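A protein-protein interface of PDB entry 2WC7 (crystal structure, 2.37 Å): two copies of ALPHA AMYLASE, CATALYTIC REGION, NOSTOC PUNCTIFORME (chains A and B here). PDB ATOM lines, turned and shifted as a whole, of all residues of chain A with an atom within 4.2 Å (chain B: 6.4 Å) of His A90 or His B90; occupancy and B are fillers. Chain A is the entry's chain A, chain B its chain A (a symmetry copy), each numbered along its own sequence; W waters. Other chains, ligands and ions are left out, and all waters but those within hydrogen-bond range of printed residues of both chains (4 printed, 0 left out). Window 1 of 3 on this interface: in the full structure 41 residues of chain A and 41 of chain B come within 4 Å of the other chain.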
ATOM      1  N   GLN A  80     -24.153  12.413  25.161  1.00  0.00           N
ATOM      2  CA  GLN A  80     -24.038  11.039  25.638  1.00  0.00           C
ATOM      3  C   GLN A  80     -22.708  10.812  26.349  1.00  0.00           C
ATOM      4  O   GLN A  80     -21.646  11.139  25.818  1.00  0.00           O
ATOM      5  CB  GLN A  80     -24.188  10.055  24.476  1.00  0.00           C
ATOM      6  CG  GLN A  80     -24.305   8.602  24.905  1.00  0.00           C
ATOM      7  CD  GLN A  80     -24.531   7.665  23.735  1.00  0.00           C
ATOM      8  OE1 GLN A  80     -23.580   7.180  23.121  1.00  0.00           O
ATOM      9  NE2 GLN A  80     -25.794   7.404  23.420  1.00  0.00           N
ATOM     10  N   SER A  81     -22.774  10.251  27.552  1.00  0.00           N
ATOM     11  CA  SER A  81     -21.587  10.001  28.340  1.00  0.00           C
ATOM     12  C   SER A  81     -21.968   9.067  29.476  1.00  0.00           C
ATOM     13  O   SER A  81     -23.149   8.879  29.756  1.00  0.00           O
ATOM     14  CB  SER A  81     -21.061  11.328  28.884  1.00  0.00           C
ATOM     15  OG  SER A  81     -22.110  12.078  29.484  1.00  0.00           O
ATOM     16  N   HIS A  88     -17.012  13.448  30.253  1.00  0.00           N
ATOM     17  CA  HIS A  88     -16.252  12.423  29.526  1.00  0.00           C
ATOM     18  C   HIS A  88     -17.174  12.013  28.371  1.00  0.00           C
ATOM     19  O   HIS A  88     -17.900  11.025  28.470  1.00  0.00           O
ATOM     20  CB  HIS A  88     -15.988  11.189  30.402  1.00  0.00           C
ATOM     21  CG  HIS A  88     -15.349  11.490  31.725  1.00  0.00           C
ATOM     22  ND1 HIS A  88     -14.853  10.501  32.549  1.00  0.00           N
ATOM     23  CD2 HIS A  88     -15.125  12.661  32.369  1.00  0.00           C
ATOM     24  CE1 HIS A  88     -14.352  11.049  33.640  1.00  0.00           C
ATOM     25  NE2 HIS A  88     -14.504  12.358  33.556  1.00  0.00           N
ATOM     26  N   THR A  89     -17.145  12.784  27.289  1.00  0.00           N
ATOM     27  CA  THR A  89     -17.996  12.545  26.136  1.00  0.00           C
ATOM     28  C   THR A  89     -17.792  11.211  25.434  1.00  0.00           C
ATOM     29  O   THR A  89     -16.661  10.805  25.153  1.00  0.00           O
ATOM     30  CB  THR A  89     -17.812  13.657  25.102  1.00  0.00           C
ATOM     31  OG1 THR A  89     -17.930  14.925  25.756  1.00  0.00           O
ATOM     32  CG2 THR A  89     -18.868  13.557  24.011  1.00  0.00           C
ATOM     33  N   HIS A  90     -18.904  10.537  25.154  1.00  0.00           N
ATOM     34  CA  HIS A  90     -18.875   9.262  24.451  1.00  0.00           C
ATOM     35  C   HIS A  90     -19.236   9.497  22.990  1.00  0.00           C
ATOM     36  O   HIS A  90     -18.528   9.056  22.092  1.00  0.00           O
ATOM     37  CB  HIS A  90     -19.857   8.266  25.074  1.00  0.00           C
ATOM     38  CG  HIS A  90     -19.908   6.957  24.351  1.00  0.00           C
ATOM     39  ND1 HIS A  90     -20.729   6.738  23.266  1.00  0.00           N
ATOM     40  CD2 HIS A  90     -19.190   5.821  24.516  1.00  0.00           C
ATOM     41  CE1 HIS A  90     -20.514   5.522  22.794  1.00  0.00           C
ATOM     42  NE2 HIS A  90     -19.583   4.946  23.534  1.00  0.00           N
ATOM     43  N   ASP A  91     -20.349  10.181  22.765  1.00  0.00           N
ATOM     44  CA  ASP A  91     -20.796  10.513  21.418  1.00  0.00           C
ATOM     45  C   ASP A  91     -21.268  11.969  21.432  1.00  0.00           C
ATOM     46  O   ASP A  91     -22.243  12.292  22.099  1.00  0.00           O
ATOM     47  CB  ASP A  91     -21.956   9.607  20.995  1.00  0.00           C
ATOM     48  CG  ASP A  91     -22.393   9.850  19.555  1.00  0.00           C
ATOM     49  OD1 ASP A  91     -23.467   9.354  19.162  1.00  0.00           O
ATOM     50  OD2 ASP A  91     -21.662  10.526  18.809  1.00  0.00           O
ATOM     51  N   SER A 129     -13.378  10.464  26.139  1.00  0.00           N
ATOM     52  CA  SER A 129     -13.550   9.366  27.081  1.00  0.00           C
ATOM     53  C   SER A 129     -12.921   8.123  26.471  1.00  0.00           C
ATOM     54  O   SER A 129     -12.425   8.172  25.349  1.00  0.00           O
ATOM     55  CB  SER A 129     -15.034   9.101  27.324  1.00  0.00           C
ATOM     56  OG  SER A 129     -15.636   8.438  26.220  1.00  0.00           O
ATOM     57  N   GLY A 131     -14.590   5.504  25.739  1.00  0.00           N
ATOM     58  CA  GLY A 131     -15.589   4.895  24.882  1.00  0.00           C
ATOM     59  C   GLY A 131     -15.758   5.621  23.567  1.00  0.00           C
ATOM     60  O   GLY A 131     -16.278   5.054  22.604  1.00  0.00           O
ATOM     61  N   PHE A 132     -15.333   6.885  23.532  1.00  0.00           N
ATOM     62  CA  PHE A 132     -15.416   7.702  22.322  1.00  0.00           C
ATOM     63  C   PHE A 132     -14.871   6.842  21.177  1.00  0.00           C
ATOM     64  O   PHE A 132     -13.727   6.393  21.224  1.00  0.00           O
ATOM     65  CB  PHE A 132     -14.580   8.978  22.509  1.00  0.00           C
ATOM     66  CG  PHE A 132     -14.469   9.823  21.274  1.00  0.00           C
ATOM     67  CD1 PHE A 132     -15.575  10.512  20.780  1.00  0.00           C
ATOM     68  CD2 PHE A 132     -13.260   9.924  20.599  1.00  0.00           C
ATOM     69  CE1 PHE A 132     -15.475  11.291  19.628  1.00  0.00           C
ATOM     70  CE2 PHE A 132     -13.150  10.697  19.448  1.00  0.00           C
ATOM     71  CZ  PHE A 132     -14.258  11.384  18.960  1.00  0.00           C
ATOM     72  N   PHE A 133     -15.690   6.622  20.154  1.00  0.00           N
ATOM     73  CA  PHE A 133     -15.317   5.759  19.035  1.00  0.00           C
ATOM     74  C   PHE A 133     -13.869   5.696  18.552  1.00  0.00           C
ATOM     75  O   PHE A 133     -13.277   4.615  18.530  1.00  0.00           O
ATOM     76  CB  PHE A 133     -16.193   6.013  17.808  1.00  0.00           C
ATOM     77  CG  PHE A 133     -15.856   5.103  16.658  1.00  0.00           C
ATOM     78  CD1 PHE A 133     -15.972   3.719  16.802  1.00  0.00           C
ATOM     79  CD2 PHE A 133     -15.338   5.612  15.473  1.00  0.00           C
ATOM     80  CE1 PHE A 133     -15.575   2.854  15.792  1.00  0.00           C
ATOM     81  CE2 PHE A 133     -14.934   4.753  14.446  1.00  0.00           C
ATOM     82  CZ  PHE A 133     -15.051   3.367  14.608  1.00  0.00           C
ATOM     83  N   HIS A 136     -11.698   4.410  21.091  1.00  0.00           N
ATOM     84  CA  HIS A 136     -12.064   3.004  21.231  1.00  0.00           C
ATOM     85  C   HIS A 136     -11.220   2.192  20.245  1.00  0.00           C
ATOM     86  O   HIS A 136     -10.607   1.188  20.602  1.00  0.00           O
ATOM     87  CB  HIS A 136     -13.543   2.812  20.894  1.00  0.00           C
ATOM     88  CG  HIS A 136     -13.932   1.383  20.655  1.00  0.00           C
ATOM     89  ND1 HIS A 136     -14.081   0.468  21.675  1.00  0.00           N
ATOM     90  CD2 HIS A 136     -14.185   0.709  19.506  1.00  0.00           C
ATOM     91  CE1 HIS A 136     -14.407  -0.707  21.166  1.00  0.00           C
ATOM     92  NE2 HIS A 136     -14.477  -0.589  19.853  1.00  0.00           N
ATOM     93  N   PHE B  79     -21.953  -1.767  10.360  1.00  0.00           N
ATOM     94  CA  PHE B  79     -22.182  -0.735  11.363  1.00  0.00           C
ATOM     95  C   PHE B  79     -20.873  -0.298  12.014  1.00  0.00           C
ATOM     96  O   PHE B  79     -19.892  -1.041  12.016  1.00  0.00           O
ATOM     97  CB  PHE B  79     -23.159  -1.231  12.431  1.00  0.00           C
ATOM     98  CG  PHE B  79     -24.547  -1.477  11.914  1.00  0.00           C
ATOM     99  CD1 PHE B  79     -25.347  -2.460  12.476  1.00  0.00           C
ATOM    100  CD2 PHE B  79     -25.054  -0.727  10.867  1.00  0.00           C
ATOM    101  CE1 PHE B  79     -26.625  -2.689  12.003  1.00  0.00           C
ATOM    102  CE2 PHE B  79     -26.332  -0.952  10.388  1.00  0.00           C
ATOM    103  CZ  PHE B  79     -27.118  -1.933  10.958  1.00  0.00           C
ATOM    104  N   GLN B  80     -20.866   0.911  12.565  1.00  0.00           N
ATOM    105  CA  GLN B  80     -19.665   1.467  13.178  1.00  0.00           C
ATOM    106  C   GLN B  80     -19.008   0.458  14.114  1.00  0.00           C
ATOM    107  O   GLN B  80     -19.665  -0.121  14.980  1.00  0.00           O
ATOM    108  CB  GLN B  80     -19.999   2.751  13.940  1.00  0.00           C
ATOM    109  CG  GLN B  80     -18.780   3.520  14.423  1.00  0.00           C
ATOM    110  CD  GLN B  80     -19.146   4.824  15.104  1.00  0.00           C
ATOM    111  OE1 GLN B  80     -19.379   4.863  16.312  1.00  0.00           O
ATOM    112  NE2 GLN B  80     -19.197   5.902  14.330  1.00  0.00           N
ATOM    113  N   SER B  81     -17.708   0.252  13.934  1.00  0.00           N
ATOM    114  CA  SER B  81     -16.969  -0.695  14.741  1.00  0.00           C
ATOM    115  C   SER B  81     -15.487  -0.445  14.517  1.00  0.00           C
ATOM    116  O   SER B  81     -15.109   0.242  13.571  1.00  0.00           O
ATOM    117  CB  SER B  81     -17.348  -2.113  14.318  1.00  0.00           C
ATOM    118  OG  SER B  81     -17.281  -2.252  12.904  1.00  0.00           O
ATOM    119  N   ALA B  82     -14.646  -0.982  15.391  1.00  0.00           N
ATOM    120  CA  ALA B  82     -13.212  -0.792  15.237  1.00  0.00           C
ATOM    121  C   ALA B  82     -12.742  -1.413  13.921  1.00  0.00           C
ATOM    122  O   ALA B  82     -13.387  -2.312  13.397  1.00  0.00           O
ATOM    123  CB  ALA B  82     -12.478  -1.423  16.412  1.00  0.00           C
ATOM    124  N   HIS B  88     -17.667  -6.551  16.039  1.00  0.00           N
ATOM    125  CA  HIS B  88     -17.661  -6.003  17.402  1.00  0.00           C
ATOM    126  C   HIS B  88     -18.305  -4.619  17.258  1.00  0.00           C
ATOM    127  O   HIS B  88     -17.609  -3.613  17.135  1.00  0.00           O
ATOM    128  CB  HIS B  88     -16.229  -5.822  17.930  1.00  0.00           C
ATOM    129  CG  HIS B  88     -15.375  -7.052  17.845  1.00  0.00           C
ATOM    130  ND1 HIS B  88     -14.140  -7.139  18.454  1.00  0.00           N
ATOM    131  CD2 HIS B  88     -15.571  -8.240  17.224  1.00  0.00           C
ATOM    132  CE1 HIS B  88     -13.614  -8.325  18.214  1.00  0.00           C
ATOM    133  NE2 HIS B  88     -14.461  -9.013  17.471  1.00  0.00           N
ATOM    134  N   THR B  89     -19.634  -4.583  17.264  1.00  0.00           N
ATOM    135  CA  THR B  89     -20.382  -3.349  17.092  1.00  0.00           C
ATOM    136  C   THR B  89     -20.150  -2.286  18.155  1.00  0.00           C
ATOM    137  O   THR B  89     -20.172  -2.570  19.355  1.00  0.00           O
ATOM    138  CB  THR B  89     -21.883  -3.644  17.036  1.00  0.00           C
ATOM    139  OG1 THR B  89     -22.117  -4.692  16.090  1.00  0.00           O
ATOM    140  CG2 THR B  89     -22.658  -2.405  16.610  1.00  0.00           C
ATOM    141  N   HIS B  90     -19.931  -1.057  17.695  1.00  0.00           N
ATOM    142  CA  HIS B  90     -19.729   0.075  18.589  1.00  0.00           C
ATOM    143  C   HIS B  90     -21.026   0.869  18.677  1.00  0.00           C
ATOM    144  O   HIS B  90     -21.504   1.168  19.766  1.00  0.00           O
ATOM    145  CB  HIS B  90     -18.600   0.979  18.089  1.00  0.00           C
ATOM    146  CG  HIS B  90     -18.392   2.189  18.943  1.00  0.00           C
ATOM    147  ND1 HIS B  90     -19.099   3.359  18.761  1.00  0.00           N
ATOM    148  CD2 HIS B  90     -17.602   2.389  20.025  1.00  0.00           C
ATOM    149  CE1 HIS B  90     -18.754   4.227  19.697  1.00  0.00           C
ATOM    150  NE2 HIS B  90     -17.850   3.662  20.477  1.00  0.00           N
ATOM    151  N   ASP B  91     -21.576   1.220  17.524  1.00  0.00           N
ATOM    152  CA  ASP B  91     -22.838   1.949  17.456  1.00  0.00           C
ATOM    153  C   ASP B  91     -23.682   1.312  16.352  1.00  0.00           C
ATOM    154  O   ASP B  91     -23.309   1.363  15.185  1.00  0.00           O
ATOM    155  CB  ASP B  91     -22.592   3.423  17.122  1.00  0.00           C
ATOM    156  CG  ASP B  91     -23.872   4.249  17.139  1.00  0.00           C
ATOM    157  OD1 ASP B  91     -23.852   5.400  16.659  1.00  0.00           O
ATOM    158  OD2 ASP B  91     -24.901   3.757  17.639  1.00  0.00           O
ATOM    159  N   TYR B  92     -24.813   0.708  16.714  1.00  0.00           N
ATOM    160  CA  TYR B  92     -25.686   0.070  15.720  1.00  0.00           C
ATOM    161  C   TYR B  92     -26.463   1.057  14.848  1.00  0.00           C
ATOM    162  O   TYR B  92     -26.944   0.697  13.772  1.00  0.00           O
ATOM    163  CB  TYR B  92     -26.701  -0.851  16.397  1.00  0.00           C
ATOM    164  CG  TYR B  92     -26.120  -2.084  17.042  1.00  0.00           C
ATOM    165  CD1 TYR B  92     -25.607  -2.041  18.335  1.00  0.00           C
ATOM    166  CD2 TYR B  92     -26.097  -3.304  16.361  1.00  0.00           C
ATOM    167  CE1 TYR B  92     -25.087  -3.182  18.938  1.00  0.00           C
ATOM    168  CE2 TYR B  92     -25.583  -4.450  16.952  1.00  0.00           C
ATOM    169  CZ  TYR B  92     -25.079  -4.385  18.239  1.00  0.00           C
ATOM    170  OH  TYR B  92     -24.554  -5.512  18.827  1.00  0.00           O
ATOM    171  N   SER B 128     -21.714  -7.159  21.516  1.00  0.00           N
ATOM    172  CA  SER B 128     -21.297  -5.892  20.920  1.00  0.00           C
ATOM    173  C   SER B 128     -19.781  -5.655  20.905  1.00  0.00           C
ATOM    174  O   SER B 128     -19.074  -6.215  20.065  1.00  0.00           O
ATOM    175  CB  SER B 128     -22.011  -4.724  21.622  1.00  0.00           C
ATOM    176  OG  SER B 128     -21.787  -4.733  23.022  1.00  0.00           O
ATOM    177  N   SER B 129     -19.295  -4.815  21.816  1.00  0.00           N
ATOM    178  CA  SER B 129     -17.876  -4.491  21.907  1.00  0.00           C
ATOM    179  C   SER B 129     -17.641  -3.786  23.233  1.00  0.00           C
ATOM    180  O   SER B 129     -18.584  -3.556  23.984  1.00  0.00           O
ATOM    181  CB  SER B 129     -17.471  -3.555  20.770  1.00  0.00           C
ATOM    182  OG  SER B 129     -17.935  -2.231  20.991  1.00  0.00           O
ATOM    183  N   ARG B 130     -16.391  -3.433  23.521  1.00  0.00           N
ATOM    184  CA  ARG B 130     -16.074  -2.744  24.772  1.00  0.00           C
ATOM    185  C   ARG B 130     -16.374  -1.251  24.670  1.00  0.00           C
ATOM    186  O   ARG B 130     -16.404  -0.546  25.680  1.00  0.00           O
ATOM    187  CB  ARG B 130     -14.598  -2.920  25.140  1.00  0.00           C
ATOM    188  CG  ARG B 130     -14.190  -4.323  25.529  1.00  0.00           C
ATOM    189  CD  ARG B 130     -13.256  -4.857  24.486  1.00  0.00           C
ATOM    190  NE  ARG B 130     -11.992  -5.337  25.023  1.00  0.00           N
ATOM    191  CZ  ARG B 130     -10.930  -5.591  24.267  1.00  0.00           C
ATOM    192  NH1 ARG B 130     -10.990  -5.401  22.959  1.00  0.00           N
ATOM    193  NH2 ARG B 130      -9.812  -6.044  24.812  1.00  0.00           N
ATOM    194  N   GLY B 131     -16.596  -0.779  23.448  1.00  0.00           N
ATOM    195  CA  GLY B 131     -16.881   0.628  23.241  1.00  0.00           C
ATOM    196  C   GLY B 131     -18.362   0.928  23.188  1.00  0.00           C
ATOM    197  O   GLY B 131     -18.773   2.074  23.380  1.00  0.00           O
ATOM    198  N   PHE B 132     -19.163  -0.103  22.913  1.00  0.00           N
ATOM    199  CA  PHE B 132     -20.618   0.036  22.849  1.00  0.00           C
ATOM    200  C   PHE B 132     -21.036   0.817  24.098  1.00  0.00           C
ATOM    201  O   PHE B 132     -20.769   0.390  25.220  1.00  0.00           O
ATOM    202  CB  PHE B 132     -21.262  -1.358  22.820  1.00  0.00           C
ATOM    203  CG  PHE B 132     -22.760  -1.341  22.906  1.00  0.00           C
ATOM    204  CD1 PHE B 132     -23.530  -0.865  21.846  1.00  0.00           C
ATOM    205  CD2 PHE B 132     -23.403  -1.794  24.050  1.00  0.00           C
ATOM    206  CE1 PHE B 132     -24.921  -0.841  21.929  1.00  0.00           C
ATOM    207  CE2 PHE B 132     -24.791  -1.774  24.142  1.00  0.00           C
ATOM    208  CZ  PHE B 132     -25.554  -1.297  23.081  1.00  0.00           C
ATOM    209  N   PHE B 133     -21.694   1.955  23.899  1.00  0.00           N
ATOM    210  CA  PHE B 133     -22.083   2.828  25.004  1.00  0.00           C
ATOM    211  C   PHE B 133     -22.482   2.239  26.355  1.00  0.00           C
ATOM    212  O   PHE B 133     -21.873   2.573  27.374  1.00  0.00           O
ATOM    213  CB  PHE B 133     -23.186   3.804  24.591  1.00  0.00           C
ATOM    214  CG  PHE B 133     -23.572   4.745  25.701  1.00  0.00           C
ATOM    215  CD1 PHE B 133     -22.622   5.611  26.247  1.00  0.00           C
ATOM    216  CD2 PHE B 133     -24.841   4.703  26.263  1.00  0.00           C
ATOM    217  CE1 PHE B 133     -22.924   6.417  27.336  1.00  0.00           C
ATOM    218  CE2 PHE B 133     -25.162   5.511  27.359  1.00  0.00           C
ATOM    219  CZ  PHE B 133     -24.198   6.369  27.899  1.00  0.00           C
ATOM    220  N   PHE B 134     -23.498   1.386  26.387  1.00  0.00           N
ATOM    221  CA  PHE B 134     -23.938   0.840  27.663  1.00  0.00           C
ATOM    222  C   PHE B 134     -22.925  -0.062  28.346  1.00  0.00           C
ATOM    223  O   PHE B 134     -22.893  -0.136  29.573  1.00  0.00           O
ATOM    224  CB  PHE B 134     -25.286   0.160  27.493  1.00  0.00           C
ATOM    225  CG  PHE B 134     -26.329   1.077  26.939  1.00  0.00           C
ATOM    226  CD1 PHE B 134     -26.650   1.051  25.585  1.00  0.00           C
ATOM    227  CD2 PHE B 134     -26.926   2.033  27.754  1.00  0.00           C
ATOM    228  CE1 PHE B 134     -27.551   1.972  25.049  1.00  0.00           C
ATOM    229  CE2 PHE B 134     -27.828   2.956  27.235  1.00  0.00           C
ATOM    230  CZ  PHE B 134     -28.142   2.931  25.877  1.00  0.00           C
ATOM    231  N   HIS B 136     -19.757   0.482  27.873  1.00  0.00           N
ATOM    232  CA  HIS B 136     -18.789   1.515  28.231  1.00  0.00           C
ATOM    233  C   HIS B 136     -19.120   2.007  29.642  1.00  0.00           C
ATOM    234  O   HIS B 136     -18.254   2.092  30.510  1.00  0.00           O
ATOM    235  CB  HIS B 136     -18.891   2.690  27.258  1.00  0.00           C
ATOM    236  CG  HIS B 136     -18.212   3.938  27.738  1.00  0.00           C
ATOM    237  ND1 HIS B 136     -16.843   4.094  27.729  1.00  0.00           N
ATOM    238  CD2 HIS B 136     -18.718   5.082  28.259  1.00  0.00           C
ATOM    239  CE1 HIS B 136     -16.533   5.279  28.224  1.00  0.00           C
ATOM    240  NE2 HIS B 136     -17.652   5.900  28.552  1.00  0.00           N
HETATM  241  O   HOH W   1     -23.793   5.376  20.447  1.00  0.00           O
HETATM  242  O   HOH W   2     -15.109  -2.591  17.765  1.00  0.00           O
HETATM  243  O   HOH W   3     -20.428   7.451  17.941  1.00  0.00           O
HETATM  244  O   HOH W   4     -18.098   8.572  29.747  1.00  0.00           O
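Gln A80 touches Phe B133, and with the chains exchanged Phe A133 touches Gln B80. Ser A81 touches Phe B133, and with the chains exchanged Phe A133 touches Ser B81. His A90 touches its own counterpart, His B90. Gly A131 touches its own counterpart, Gly B131. 11 positions are printed for both chains. Of the 17 pairs that touch across the chains among the printed residues, 16 have their exchanged pair printed and touching as well.
Water W4 bridges O of His A88 (2.8 Å) and NE2 of His B136 (3.0 Å). Water W2 lies within hydrogen-bond range of O of His B88 (2.8 Å), N of Ala B82 (2.9 Å) and NE2 of His A136 (3.0 Å). Water W1 bridges the side-chain amide oxygen (OE1) of Gln A80 (3.2 Å) and the side-chain carboxylate (OD2) of Asp B91 (3.4 Å). Water W3 lies within hydrogen-bond range of the side-chain amide oxygen (OE1) of Gln B80 (3.2 Å) and the side-chain carboxylate (OD2) of Asp A91 (3.4 Å).
Hydrophobic or aromatic side chains of chain B that line the printed part of chain A: His B90, Phe B133 and His B136. Along chain B the printed residues that touch a printed residue of chain A span positions 80 to 136. Of the 11 printed residues of chain A, 7 touch a printed residue of chain B. Hydrophobic or aromatic side chains of chain A that line the printed part of chain B: His A90, Phe A133 and His A136.
O of Thr A89 sits at hydrogen-bond distance from OG of Ser A129 (2.8 Å). The side-chain hydroxyl (OG) of Ser B129 sits at hydrogen-bond distance from the backbone NH (N) of Phe B132 (3.1 Å). The backbone carbonyl oxygen (O) of Thr B89 is in hydrogen-bond range of the side-chain hydroxyl (OG) of Ser B129 (2.8 Å). The side-chain hydroxyl (OG) of Ser A129 is in hydrogen-bond range of the backbone NH (N) of Gly A131 (3.2 Å). The backbone carbonyl oxygen (O) of Gly A131 lies within hydrogen-bond range of a ring nitrogen (NE2) of His A90. The backbone carbonyl oxygen (O) of Gln B80 is in hydrogen-bond range of the backbone NH (N) of His B90 (2.9 Å).
Among the printed residues, pairs that only touch across the chains: Phe A133 with Ser B81, Ser A81 with Phe B133, Gln A80 with Phe B133, Phe A133 with Gln B80, His A90 with Phe B133, Phe A133 with His B90, His A90 with His B90, His A136 with His B90, His A90 with His B136, Ser A129 with His B136, His A136 with Ser B129, Gly A131 with Gly B131 and Phe A133 with Ala B82.
A ring nitrogen (NE2) of His B90 sits at hydrogen-bond distance from the backbone carbonyl oxygen of Gly A131 (3.0 Å). ND1 of His A136 lies close to N of Gly B131. A ring nitrogen (ND1) of His B136 lies close to the backbone NH of Gly A131 (3.3 Å). A ring nitrogen (NE2) of His A90 is in hydrogen-bond range of the backbone carbonyl oxygen (O) of Gly B131, at 3.0 Å.
Of the printed residues of chain B, Gln A80 touches Phe B133. Of the printed residues of chain B, His A90 touches His B90 (3.7 Å), Gly B131 (3.0 Å), Phe B133 (3.6 Å) and His B136 (3.8 Å). Of the printed residues of chain A, Phe B133 touches Gln A80 (3.5 Å), Ser A81 (3.3 Å) and His A90 (3.6 Å). Of the printed residues of chain A, His B136 touches His A90 (3.8 Å), Ser A129 (3.8 Å) and Gly A131 (3.2 Å). The nearest printed residue of chain A that does not touch His B90 is Phe A132 (4.4 Å). The nearest printed residue of chain B that does not touch Gln A80 is Phe B134 (5.6 Å).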
